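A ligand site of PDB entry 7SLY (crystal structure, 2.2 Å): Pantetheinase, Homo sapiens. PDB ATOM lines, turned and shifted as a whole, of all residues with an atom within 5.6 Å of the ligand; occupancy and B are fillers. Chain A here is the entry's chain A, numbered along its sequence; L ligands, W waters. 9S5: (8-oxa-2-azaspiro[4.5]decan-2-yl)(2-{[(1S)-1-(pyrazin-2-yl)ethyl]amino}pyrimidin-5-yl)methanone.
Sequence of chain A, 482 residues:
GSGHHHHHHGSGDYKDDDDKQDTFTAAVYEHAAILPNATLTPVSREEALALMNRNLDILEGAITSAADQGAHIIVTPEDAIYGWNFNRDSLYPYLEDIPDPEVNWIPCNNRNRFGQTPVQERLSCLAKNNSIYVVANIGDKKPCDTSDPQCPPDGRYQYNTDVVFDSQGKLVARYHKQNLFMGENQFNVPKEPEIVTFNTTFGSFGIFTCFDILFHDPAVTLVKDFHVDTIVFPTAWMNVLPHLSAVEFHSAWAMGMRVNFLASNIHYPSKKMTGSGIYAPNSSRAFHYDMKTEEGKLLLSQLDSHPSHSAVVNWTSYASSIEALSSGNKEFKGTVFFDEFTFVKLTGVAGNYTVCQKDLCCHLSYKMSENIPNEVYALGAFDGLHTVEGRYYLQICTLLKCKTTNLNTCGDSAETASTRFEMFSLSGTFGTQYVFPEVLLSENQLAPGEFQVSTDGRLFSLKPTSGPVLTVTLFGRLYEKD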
ATOM      1  N   GLU A  78     -26.054  23.897  13.903  1.00  0.00           N
ATOM      2  CA  GLU A  78     -26.639  23.466  15.172  1.00  0.00           C
ATOM      3  C   GLU A  78     -25.485  23.125  16.121  1.00  0.00           C
ATOM      4  O   GLU A  78     -24.471  22.579  15.647  1.00  0.00           O
ATOM      5  CB  GLU A  78     -27.479  22.213  14.967  1.00  0.00           C
ATOM      6  CG  GLU A  78     -28.086  21.631  16.226  1.00  0.00           C
ATOM      7  CD  GLU A  78     -28.609  20.227  16.013  1.00  0.00           C
ATOM      8  OE1 GLU A  78     -28.117  19.567  15.074  1.00  0.00           O
ATOM      9  OE2 GLU A  78     -29.532  19.802  16.748  1.00  0.00           O
ATOM     10  N   ASP A  79     -25.628  23.440  17.432  1.00  0.00           N
ATOM     11  CA  ASP A  79     -24.586  23.180  18.435  1.00  0.00           C
ATOM     12  C   ASP A  79     -23.243  23.871  18.187  1.00  0.00           C
ATOM     13  O   ASP A  79     -22.268  23.525  18.830  1.00  0.00           O
ATOM     14  CB  ASP A  79     -24.366  21.661  18.609  1.00  0.00           C
ATOM     15  CG  ASP A  79     -25.549  20.966  19.231  1.00  0.00           C
ATOM     16  OD1 ASP A  79     -26.442  21.674  19.759  1.00  0.00           O
ATOM     17  OD2 ASP A  79     -25.589  19.730  19.185  1.00  0.00           O
ATOM     18  N   TRP A  84     -22.118  19.220  21.632  1.00  0.00           N
ATOM     19  CA  TRP A  84     -23.160  18.224  21.883  1.00  0.00           C
ATOM     20  C   TRP A  84     -22.897  17.192  23.035  1.00  0.00           C
ATOM     21  O   TRP A  84     -23.658  16.224  23.149  1.00  0.00           O
ATOM     22  CB  TRP A  84     -23.396  17.463  20.566  1.00  0.00           C
ATOM     23  CG  TRP A  84     -22.107  16.973  19.950  1.00  0.00           C
ATOM     24  CD1 TRP A  84     -21.423  15.834  20.269  1.00  0.00           C
ATOM     25  CD2 TRP A  84     -21.310  17.660  18.975  1.00  0.00           C
ATOM     26  NE1 TRP A  84     -20.237  15.778  19.568  1.00  0.00           N
ATOM     27  CE2 TRP A  84     -20.150  16.888  18.758  1.00  0.00           C
ATOM     28  CE3 TRP A  84     -21.454  18.882  18.292  1.00  0.00           C
ATOM     29  CZ2 TRP A  84     -19.156  17.276  17.861  1.00  0.00           C
ATOM     30  CZ3 TRP A  84     -20.470  19.260  17.392  1.00  0.00           C
ATOM     31  CH2 TRP A  84     -19.323  18.474  17.196  1.00  0.00           C
ATOM     32  N   LYS A 177     -36.393  22.761  18.739  1.00  0.00           N
ATOM     33  CA  LYS A 177     -36.317  21.506  17.975  1.00  0.00           C
ATOM     34  C   LYS A 177     -37.341  20.482  18.474  1.00  0.00           C
ATOM     35  O   LYS A 177     -37.373  20.163  19.667  1.00  0.00           O
ATOM     36  CB  LYS A 177     -34.910  20.937  18.037  1.00  0.00           C
ATOM     37  CG  LYS A 177     -34.581  19.837  17.043  1.00  0.00           C
ATOM     38  CD  LYS A 177     -33.206  19.270  17.472  1.00  0.00           C
ATOM     39  CE  LYS A 177     -32.646  18.164  16.638  1.00  0.00           C
ATOM     40  NZ  LYS A 177     -31.417  17.613  17.286  1.00  0.00           N
ATOM     41  N   ASN A 179     -37.928  17.250  16.915  1.00  0.00           N
ATOM     42  CA  ASN A 179     -37.468  15.873  16.776  1.00  0.00           C
ATOM     43  C   ASN A 179     -36.098  15.671  17.331  1.00  0.00           C
ATOM     44  O   ASN A 179     -35.105  15.846  16.632  1.00  0.00           O
ATOM     45  CB  ASN A 179     -37.604  15.432  15.323  1.00  0.00           C
ATOM     46  CG  ASN A 179     -39.026  15.592  14.851  1.00  0.00           C
ATOM     47  OD1 ASN A 179     -39.902  14.813  15.230  1.00  0.00           O
ATOM     48  ND2 ASN A 179     -39.322  16.673  14.156  1.00  0.00           N
ATOM     49  N   LEU A 180     -36.038  15.307  18.596  1.00  0.00           N
ATOM     50  CA  LEU A 180     -34.750  15.050  19.237  1.00  0.00           C
ATOM     51  C   LEU A 180     -34.161  13.713  18.784  1.00  0.00           C
ATOM     52  O   LEU A 180     -34.896  12.736  18.540  1.00  0.00           O
ATOM     53  CB  LEU A 180     -34.858  15.090  20.764  1.00  0.00           C
ATOM     54  CG  LEU A 180     -35.258  16.408  21.436  1.00  0.00           C
ATOM     55  CD1 LEU A 180     -35.236  16.245  22.943  1.00  0.00           C
ATOM     56  CD2 LEU A 180     -34.332  17.552  21.053  1.00  0.00           C
ATOM     57  N   PHE A 181     -32.828  13.652  18.685  1.00  0.00           N
ATOM     58  CA  PHE A 181     -32.119  12.440  18.338  1.00  0.00           C
ATOM     59  C   PHE A 181     -31.858  11.603  19.579  1.00  0.00           C
ATOM     60  O   PHE A 181     -32.040  12.074  20.706  1.00  0.00           O
ATOM     61  CB  PHE A 181     -30.789  12.791  17.651  1.00  0.00           C
ATOM     62  CG  PHE A 181     -30.092  11.638  16.960  1.00  0.00           C
ATOM     63  CD1 PHE A 181     -30.684  10.993  15.878  1.00  0.00           C
ATOM     64  CD2 PHE A 181     -28.848  11.192  17.403  1.00  0.00           C
ATOM     65  CE1 PHE A 181     -30.023   9.940  15.222  1.00  0.00           C
ATOM     66  CE2 PHE A 181     -28.186  10.139  16.747  1.00  0.00           C
ATOM     67  CZ  PHE A 181     -28.775   9.515  15.652  1.00  0.00           C
ATOM     68  N   MET A 182     -31.444  10.350  19.354  1.00  0.00           N
ATOM     69  CA  MET A 182     -31.019   9.355  20.332  1.00  0.00           C
ATOM     70  C   MET A 182     -29.921   9.985  21.228  1.00  0.00           C
ATOM     71  O   MET A 182     -28.930  10.522  20.729  1.00  0.00           O
ATOM     72  CB  MET A 182     -30.447   8.159  19.557  1.00  0.00           C
ATOM     73  CG  MET A 182     -29.866   7.068  20.413  1.00  0.00           C
ATOM     74  SD  MET A 182     -30.047   5.466  19.610  1.00  0.00           S
ATOM     75  CE  MET A 182     -31.719   4.990  20.194  1.00  0.00           C
ATOM     76  N   GLU A 184     -30.141  12.690  23.202  1.00  0.00           N
ATOM     77  CA  GLU A 184     -30.208  14.152  23.354  1.00  0.00           C
ATOM     78  C   GLU A 184     -31.076  14.403  24.585  1.00  0.00           C
ATOM     79  O   GLU A 184     -32.128  15.062  24.517  1.00  0.00           O
ATOM     80  CB  GLU A 184     -30.787  14.824  22.102  1.00  0.00           C
ATOM     81  CG  GLU A 184     -29.808  15.659  21.301  1.00  0.00           C
ATOM     82  CD  GLU A 184     -30.439  16.479  20.191  1.00  0.00           C
ATOM     83  OE1 GLU A 184     -31.436  16.013  19.593  1.00  0.00           O
ATOM     84  OE2 GLU A 184     -29.909  17.570  19.872  1.00  0.00           O
ATOM     85  N   CYS A 210     -31.719  19.921  11.902  1.00  0.00           N
ATOM     86  CA  CYS A 210     -31.156  18.564  11.864  1.00  0.00           C
ATOM     87  C   CYS A 210     -32.159  17.460  11.550  1.00  0.00           C
ATOM     88  O   CYS A 210     -32.722  17.445  10.457  1.00  0.00           O
ATOM     89  CB  CYS A 210     -30.415  18.297  13.186  1.00  0.00           C
ATOM     90  SG  CYS A 210     -29.070  17.099  13.052  1.00  0.00           S
ATOM     91  N   PHE A 211     -32.418  16.548  12.512  1.00  0.00           N
ATOM     92  CA  PHE A 211     -33.303  15.369  12.434  1.00  0.00           C
ATOM     93  C   PHE A 211     -34.741  15.694  12.024  1.00  0.00           C
ATOM     94  O   PHE A 211     -35.459  14.811  11.541  1.00  0.00           O
ATOM     95  CB  PHE A 211     -33.298  14.659  13.797  1.00  0.00           C
ATOM     96  CG  PHE A 211     -33.648  13.183  13.864  1.00  0.00           C
ATOM     97  CD1 PHE A 211     -33.168  12.300  12.912  1.00  0.00           C
ATOM     98  CD2 PHE A 211     -34.338  12.671  14.960  1.00  0.00           C
ATOM     99  CE1 PHE A 211     -33.415  10.922  13.019  1.00  0.00           C
ATOM    100  CE2 PHE A 211     -34.607  11.288  15.060  1.00  0.00           C
ATOM    101  CZ  PHE A 211     -34.127  10.431  14.088  1.00  0.00           C
ATOM    102  N   LEU A 214     -36.244  14.636   8.724  1.00  0.00           N
ATOM    103  CA  LEU A 214     -36.792  13.267   8.482  1.00  0.00           C
ATOM    104  C   LEU A 214     -38.241  13.085   8.937  1.00  0.00           C
ATOM    105  O   LEU A 214     -38.796  11.984   8.802  1.00  0.00           O
ATOM    106  CB  LEU A 214     -35.908  12.163   9.081  1.00  0.00           C
ATOM    107  CG  LEU A 214     -34.661  11.842   8.280  1.00  0.00           C
ATOM    108  CD1 LEU A 214     -33.740  10.976   9.076  1.00  0.00           C
ATOM    109  CD2 LEU A 214     -35.013  11.122   6.949  1.00  0.00           C
ATOM    110  N   ALA A 236     -26.138  19.365  12.545  1.00  0.00           N
ATOM    111  CA  ALA A 236     -24.910  18.749  13.093  1.00  0.00           C
ATOM    112  C   ALA A 236     -25.007  17.314  12.638  1.00  0.00           C
ATOM    113  O   ALA A 236     -25.110  16.405  13.458  1.00  0.00           O
ATOM    114  CB  ALA A 236     -24.900  18.833  14.615  1.00  0.00           C
ATOM    115  N   TRP A 237     -25.023  17.127  11.317  1.00  0.00           N
ATOM    116  CA  TRP A 237     -25.339  15.875  10.657  1.00  0.00           C
ATOM    117  C   TRP A 237     -24.200  14.823  10.545  1.00  0.00           C
ATOM    118  O   TRP A 237     -23.130  15.093  10.000  1.00  0.00           O
ATOM    119  CB  TRP A 237     -25.908  16.181   9.263  1.00  0.00           C
ATOM    120  CG  TRP A 237     -26.593  15.019   8.615  1.00  0.00           C
ATOM    121  CD1 TRP A 237     -26.019  14.079   7.804  1.00  0.00           C
ATOM    122  CD2 TRP A 237     -28.005  14.752   8.613  1.00  0.00           C
ATOM    123  NE1 TRP A 237     -26.992  13.265   7.283  1.00  0.00           N
ATOM    124  CE2 TRP A 237     -28.207  13.624   7.799  1.00  0.00           C
ATOM    125  CE3 TRP A 237     -29.111  15.356   9.222  1.00  0.00           C
ATOM    126  CZ2 TRP A 237     -29.490  13.089   7.573  1.00  0.00           C
ATOM    127  CZ3 TRP A 237     -30.378  14.811   9.008  1.00  0.00           C
ATOM    128  CH2 TRP A 237     -30.558  13.716   8.181  1.00  0.00           C
ATOM    129  N   MET A 238     -24.516  13.592  10.972  1.00  0.00           N
ATOM    130  CA  MET A 238     -23.593  12.451  10.835  1.00  0.00           C
ATOM    131  C   MET A 238     -23.950  11.731   9.558  1.00  0.00           C
ATOM    132  O   MET A 238     -25.063  11.199   9.433  1.00  0.00           O
ATOM    133  CB  MET A 238     -23.699  11.500  12.031  1.00  0.00           C
ATOM    134  CG  MET A 238     -23.246  12.168  13.320  1.00  0.00           C
ATOM    135  SD  MET A 238     -23.427  11.090  14.756  1.00  0.00           S
ATOM    136  CE  MET A 238     -25.163  10.972  14.870  1.00  0.00           C
ATOM    137  N   ASN A 239     -23.036  11.778   8.578  1.00  0.00           N
ATOM    138  CA  ASN A 239     -23.212  11.182   7.263  1.00  0.00           C
ATOM    139  C   ASN A 239     -23.325   9.659   7.286  1.00  0.00           C
ATOM    140  O   ASN A 239     -22.499   8.974   7.902  1.00  0.00           O
ATOM    141  CB  ASN A 239     -22.078  11.621   6.331  1.00  0.00           C
ATOM    142  CG  ASN A 239     -21.991  13.115   6.075  1.00  0.00           C
ATOM    143  OD1 ASN A 239     -23.002  13.836   5.930  1.00  0.00           O
ATOM    144  ND2 ASN A 239     -20.765  13.570   5.913  1.00  0.00           N
ATOM    145  N   VAL A 240     -24.325   9.141   6.587  1.00  0.00           N
ATOM    146  CA  VAL A 240     -24.542   7.699   6.452  1.00  0.00           C
ATOM    147  C   VAL A 240     -24.822   7.411   4.987  1.00  0.00           C
ATOM    148  O   VAL A 240     -25.929   7.668   4.519  1.00  0.00           O
ATOM    149  CB  VAL A 240     -25.634   7.131   7.390  1.00  0.00           C
ATOM    150  CG1 VAL A 240     -26.000   5.692   7.019  1.00  0.00           C
ATOM    151  CG2 VAL A 240     -25.199   7.216   8.850  1.00  0.00           C
ATOM    152  N   LEU A 244     -27.885   8.908   3.099  1.00  0.00           N
ATOM    153  CA  LEU A 244     -28.050   9.943   4.081  1.00  0.00           C
ATOM    154  C   LEU A 244     -26.786  10.749   4.342  1.00  0.00           C
ATOM    155  O   LEU A 244     -26.494  11.126   5.486  1.00  0.00           O
ATOM    156  CB  LEU A 244     -28.688   9.371   5.347  1.00  0.00           C
ATOM    157  CG  LEU A 244     -30.185   8.980   5.147  1.00  0.00           C
ATOM    158  CD1 LEU A 244     -30.742   8.252   6.330  1.00  0.00           C
ATOM    159  CD2 LEU A 244     -31.071  10.191   4.796  1.00  0.00           C
ATOM    160  N   LYS A 271     -16.410  12.303  13.268  1.00  0.00           N
ATOM    161  CA  LYS A 271     -17.780  11.850  13.545  1.00  0.00           C
ATOM    162  C   LYS A 271     -18.587  11.825  12.246  1.00  0.00           C
ATOM    163  O   LYS A 271     -19.806  11.645  12.292  1.00  0.00           O
ATOM    164  CB  LYS A 271     -18.467  12.757  14.589  1.00  0.00           C
ATOM    165  CG  LYS A 271     -18.190  12.349  16.018  1.00  0.00           C
ATOM    166  CD  LYS A 271     -19.045  13.143  17.012  1.00  0.00           C
ATOM    167  CE  LYS A 271     -20.420  12.573  17.283  1.00  0.00           C
ATOM    168  NZ  LYS A 271     -20.361  11.387  18.186  1.00  0.00           N
ATOM    169  N   MET A 273     -19.024  14.388  10.127  1.00  0.00           N
ATOM    170  CA  MET A 273     -19.808  15.617  10.074  1.00  0.00           C
ATOM    171  C   MET A 273     -19.159  16.549   9.079  1.00  0.00           C
ATOM    172  O   MET A 273     -18.091  17.091   9.334  1.00  0.00           O
ATOM    173  CB  MET A 273     -19.937  16.281  11.462  1.00  0.00           C
ATOM    174  CG  MET A 273     -20.596  15.414  12.522  1.00  0.00           C
ATOM    175  SD  MET A 273     -20.735  16.252  14.134  1.00  0.00           S
ATOM    176  CE  MET A 273     -21.831  15.208  14.897  1.00  0.00           C
ATOM    177  N   PHE A 337     -28.033   0.652   5.620  1.00  0.00           N
ATOM    178  CA  PHE A 337     -28.305   1.338   6.902  1.00  0.00           C
ATOM    179  C   PHE A 337     -29.270   0.518   7.786  1.00  0.00           C
ATOM    180  O   PHE A 337     -30.312   1.031   8.222  1.00  0.00           O
ATOM    181  CB  PHE A 337     -28.807   2.781   6.636  1.00  0.00           C
ATOM    182  CG  PHE A 337     -28.968   3.688   7.837  1.00  0.00           C
ATOM    183  CD1 PHE A 337     -28.105   3.601   8.925  1.00  0.00           C
ATOM    184  CD2 PHE A 337     -29.934   4.694   7.841  1.00  0.00           C
ATOM    185  CE1 PHE A 337     -28.244   4.475  10.013  1.00  0.00           C
ATOM    186  CE2 PHE A 337     -30.079   5.553   8.934  1.00  0.00           C
ATOM    187  CZ  PHE A 337     -29.236   5.438  10.011  1.00  0.00           C
ATOM    188  N   HIS A 386     -37.845   1.920   9.342  1.00  0.00           N
ATOM    189  CA  HIS A 386     -36.478   2.003   9.857  1.00  0.00           C
ATOM    190  C   HIS A 386     -36.587   2.035  11.378  1.00  0.00           C
ATOM    191  O   HIS A 386     -37.520   2.639  11.900  1.00  0.00           O
ATOM    192  CB  HIS A 386     -35.763   3.282   9.374  1.00  0.00           C
ATOM    193  CG  HIS A 386     -34.325   3.337   9.798  1.00  0.00           C
ATOM    194  ND1 HIS A 386     -33.332   2.822   9.003  1.00  0.00           N
ATOM    195  CD2 HIS A 386     -33.776   3.778  10.947  1.00  0.00           C
ATOM    196  CE1 HIS A 386     -32.221   2.988   9.686  1.00  0.00           C
ATOM    197  NE2 HIS A 386     -32.443   3.538  10.861  1.00  0.00           N
ATOM    198  N   VAL A 388     -33.335   1.454  13.631  1.00  0.00           N
ATOM    199  CA  VAL A 388     -32.034   1.730  14.262  1.00  0.00           C
ATOM    200  C   VAL A 388     -31.767   3.238  14.385  1.00  0.00           C
ATOM    201  O   VAL A 388     -31.572   3.928  13.380  1.00  0.00           O
ATOM    202  CB  VAL A 388     -30.871   0.960  13.587  1.00  0.00           C
ATOM    203  CG1 VAL A 388     -29.515   1.399  14.170  1.00  0.00           C
ATOM    204  CG2 VAL A 388     -31.059  -0.557  13.712  1.00  0.00           C
ATOM    205  N   GLU A 389     -31.728   3.729  15.655  1.00  0.00           N
ATOM    206  CA  GLU A 389     -31.458   5.121  16.032  1.00  0.00           C
ATOM    207  C   GLU A 389     -32.491   6.079  15.429  1.00  0.00           C
ATOM    208  O   GLU A 389     -32.142   7.141  14.890  1.00  0.00           O
ATOM    209  CB  GLU A 389     -30.004   5.542  15.670  1.00  0.00           C
ATOM    210  CG  GLU A 389     -28.920   4.617  16.185  1.00  0.00           C
ATOM    211  CD  GLU A 389     -27.493   4.986  15.849  1.00  0.00           C
ATOM    212  OE1 GLU A 389     -27.267   6.063  15.230  1.00  0.00           O
ATOM    213  OE2 GLU A 389     -26.583   4.203  16.214  1.00  0.00           O
ATOM    214  N   GLY A 390     -33.771   5.691  15.517  1.00  0.00           N
ATOM    215  CA  GLY A 390     -34.886   6.471  15.002  1.00  0.00           C
ATOM    216  C   GLY A 390     -35.892   5.645  14.238  1.00  0.00           C
ATOM    217  O   GLY A 390     -35.493   4.816  13.426  1.00  0.00           O
ATOM    218  N   TYR A 392     -38.919   5.583  11.552  1.00  0.00           N
ATOM    219  CA  TYR A 392     -39.593   6.272  10.443  1.00  0.00           C
ATOM    220  C   TYR A 392     -39.835   5.288   9.304  1.00  0.00           C
ATOM    221  O   TYR A 392     -38.980   4.445   9.061  1.00  0.00           O
ATOM    222  CB  TYR A 392     -38.780   7.514   9.984  1.00  0.00           C
ATOM    223  CG  TYR A 392     -37.280   7.331   9.921  1.00  0.00           C
ATOM    224  CD1 TYR A 392     -36.657   6.890   8.760  1.00  0.00           C
ATOM    225  CD2 TYR A 392     -36.471   7.703  10.987  1.00  0.00           C
ATOM    226  CE1 TYR A 392     -35.278   6.768   8.675  1.00  0.00           C
ATOM    227  CE2 TYR A 392     -35.085   7.578  10.923  1.00  0.00           C
ATOM    228  CZ  TYR A 392     -34.486   7.097   9.769  1.00  0.00           C
ATOM    229  OH  TYR A 392     -33.125   6.988   9.702  1.00  0.00           O
HETATM  230  N3  9S5 L   1     -27.684  11.394  10.621  1.00  0.00           N
HETATM  231  C4  9S5 L   1     -30.544   9.135  11.023  1.00  0.00           C
HETATM  232  N2  9S5 L   1     -28.236   8.757  11.614  1.00  0.00           N
HETATM  233  C7  9S5 L   1     -27.993  12.123  11.741  1.00  0.00           C
HETATM  234  C6  9S5 L   1     -28.692   7.763  12.417  1.00  0.00           C
HETATM  235  C9  9S5 L   1     -28.593  13.661  13.901  1.00  0.00           C
HETATM  236  C13 9S5 L   1     -27.234  16.441  17.602  1.00  0.00           C
HETATM  237  C8  9S5 L   1     -29.536  12.800  13.320  1.00  0.00           C
HETATM  238  N5  9S5 L   1     -26.982  12.935  12.245  1.00  0.00           N
HETATM  239  C18 9S5 L   1     -23.950  14.398  17.506  1.00  0.00           C
HETATM  240  C16 9S5 L   1     -26.580  14.235  18.594  1.00  0.00           C
HETATM  241  C19 9S5 L   1     -24.853  15.629  17.478  1.00  0.00           C
HETATM  242  C1  9S5 L   1     -28.085   9.870   8.751  1.00  0.00           C
HETATM  243  C2  9S5 L   1     -28.696  10.527   9.986  1.00  0.00           C
HETATM  244  C3  9S5 L   1     -29.170   9.439  10.924  1.00  0.00           C
HETATM  245  N1  9S5 L   1     -30.994   8.140  11.810  1.00  0.00           N
HETATM  246  C5  9S5 L   1     -30.057   7.452  12.507  1.00  0.00           C
HETATM  247  N4  9S5 L   1     -29.291  12.029  12.249  1.00  0.00           N
HETATM  248  C10 9S5 L   1     -27.323  13.694  13.308  1.00  0.00           C
HETATM  249  C11 9S5 L   1     -29.033  14.548  14.983  1.00  0.00           C
HETATM  250  O1  9S5 L   1     -30.209  14.867  15.099  1.00  0.00           O
HETATM  251  N6  9S5 L   1     -28.098  15.092  15.860  1.00  0.00           N
HETATM  252  C12 9S5 L   1     -28.526  16.068  16.883  1.00  0.00           C
HETATM  253  C14 9S5 L   1     -26.325  15.223  17.453  1.00  0.00           C
HETATM  254  C15 9S5 L   1     -26.734  14.604  16.090  1.00  0.00           C
HETATM  255  C17 9S5 L   1     -25.567  13.091  18.574  1.00  0.00           C
HETATM  256  O2  9S5 L   1     -24.257  13.582  18.598  1.00  0.00           O
HETATM  257  O   HOH W   1     -25.596   8.322  12.428  1.00  0.00           O
HETATM  258  O   HOH W   2     -27.379  18.277  20.479  1.00  0.00           O
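O of Met 238 is in hydrogen-bond range of N3 of the ligand (2.9 Å). The side-chain hydroxyl (OH) of Tyr 392 lies within hydrogen-bond range of a nitrogen (N1) of the ligand, 3.2 Å away. The backbone NH of Met 238 is in hydrogen-bond range of a nitrogen (N5) of the ligand (2.9 Å). The side-chain sulfur (SG) of Cys 210 sits close to an oxygen (O1) of the ligand, at 3.2 Å.
NE2 of His 386 sits at hydrogen-bond distance from O of Val 388 (2.7 Å). O of Tyr 392 lies within hydrogen-bond range of N of His 386, at 2.8 Å. The backbone NH of Ala 236 is in hydrogen-bond range of the side-chain sulfur of Cys 210. The side-chain carboxylate (OE2) of Glu 78 is in salt-bridge range of the side-chain amino group (NZ) of Lys 177, at 2.9 Å. The backbone carbonyl oxygen of Leu 244 lies within hydrogen-bond range of the indole nitrogen of Trp 237 (2.8 Å). The side-chain amino group (NZ) of Lys 177 is in salt-bridge range of the side-chain carboxylate (OE1) of Glu 184 (2.8 Å). N of Phe 181 sits at hydrogen-bond distance from OE1 of Glu 184, at 2.9 Å. SG of Cys 210 lies close to OE1 of Glu 78, at 3.3 Å.
The backbone carbonyl oxygen (O) of Glu 389 sits close to a nitrogen (N1) of the ligand (3.4 Å). Merely in contact with the ligand: Lys 177 (3.3 Å), Phe 337 (3.3 Å), Phe 181 (3.3 Å), Phe 211 (3.4 Å), Met 273 (3.5 Å), Leu 244 (3.5 Å), Ala 236 (3.5 Å), Trp 237 (3.6 Å), Glu 184 (3.6 Å), Glu 78 (3.9 Å), Trp 84 (3.9 Å), Val 240 (3.9 Å), Val 388 (3.9 Å) and Lys 271 (3.98 Å). Hydrophobic or aromatic side chains that line the ligand: Trp 84, Phe 181, Phe 211, Trp 237, Met 238, Val 240, Leu 244, Met 273 and Phe 337. Of the 26 residues printed, 18 come within 4 Å of the ligand.
Water W2 lies within hydrogen-bond range of the side-chain carboxylate of Asp 79 (2.6 Å) and the side-chain carboxylate of Glu 184 (2.7 Å).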
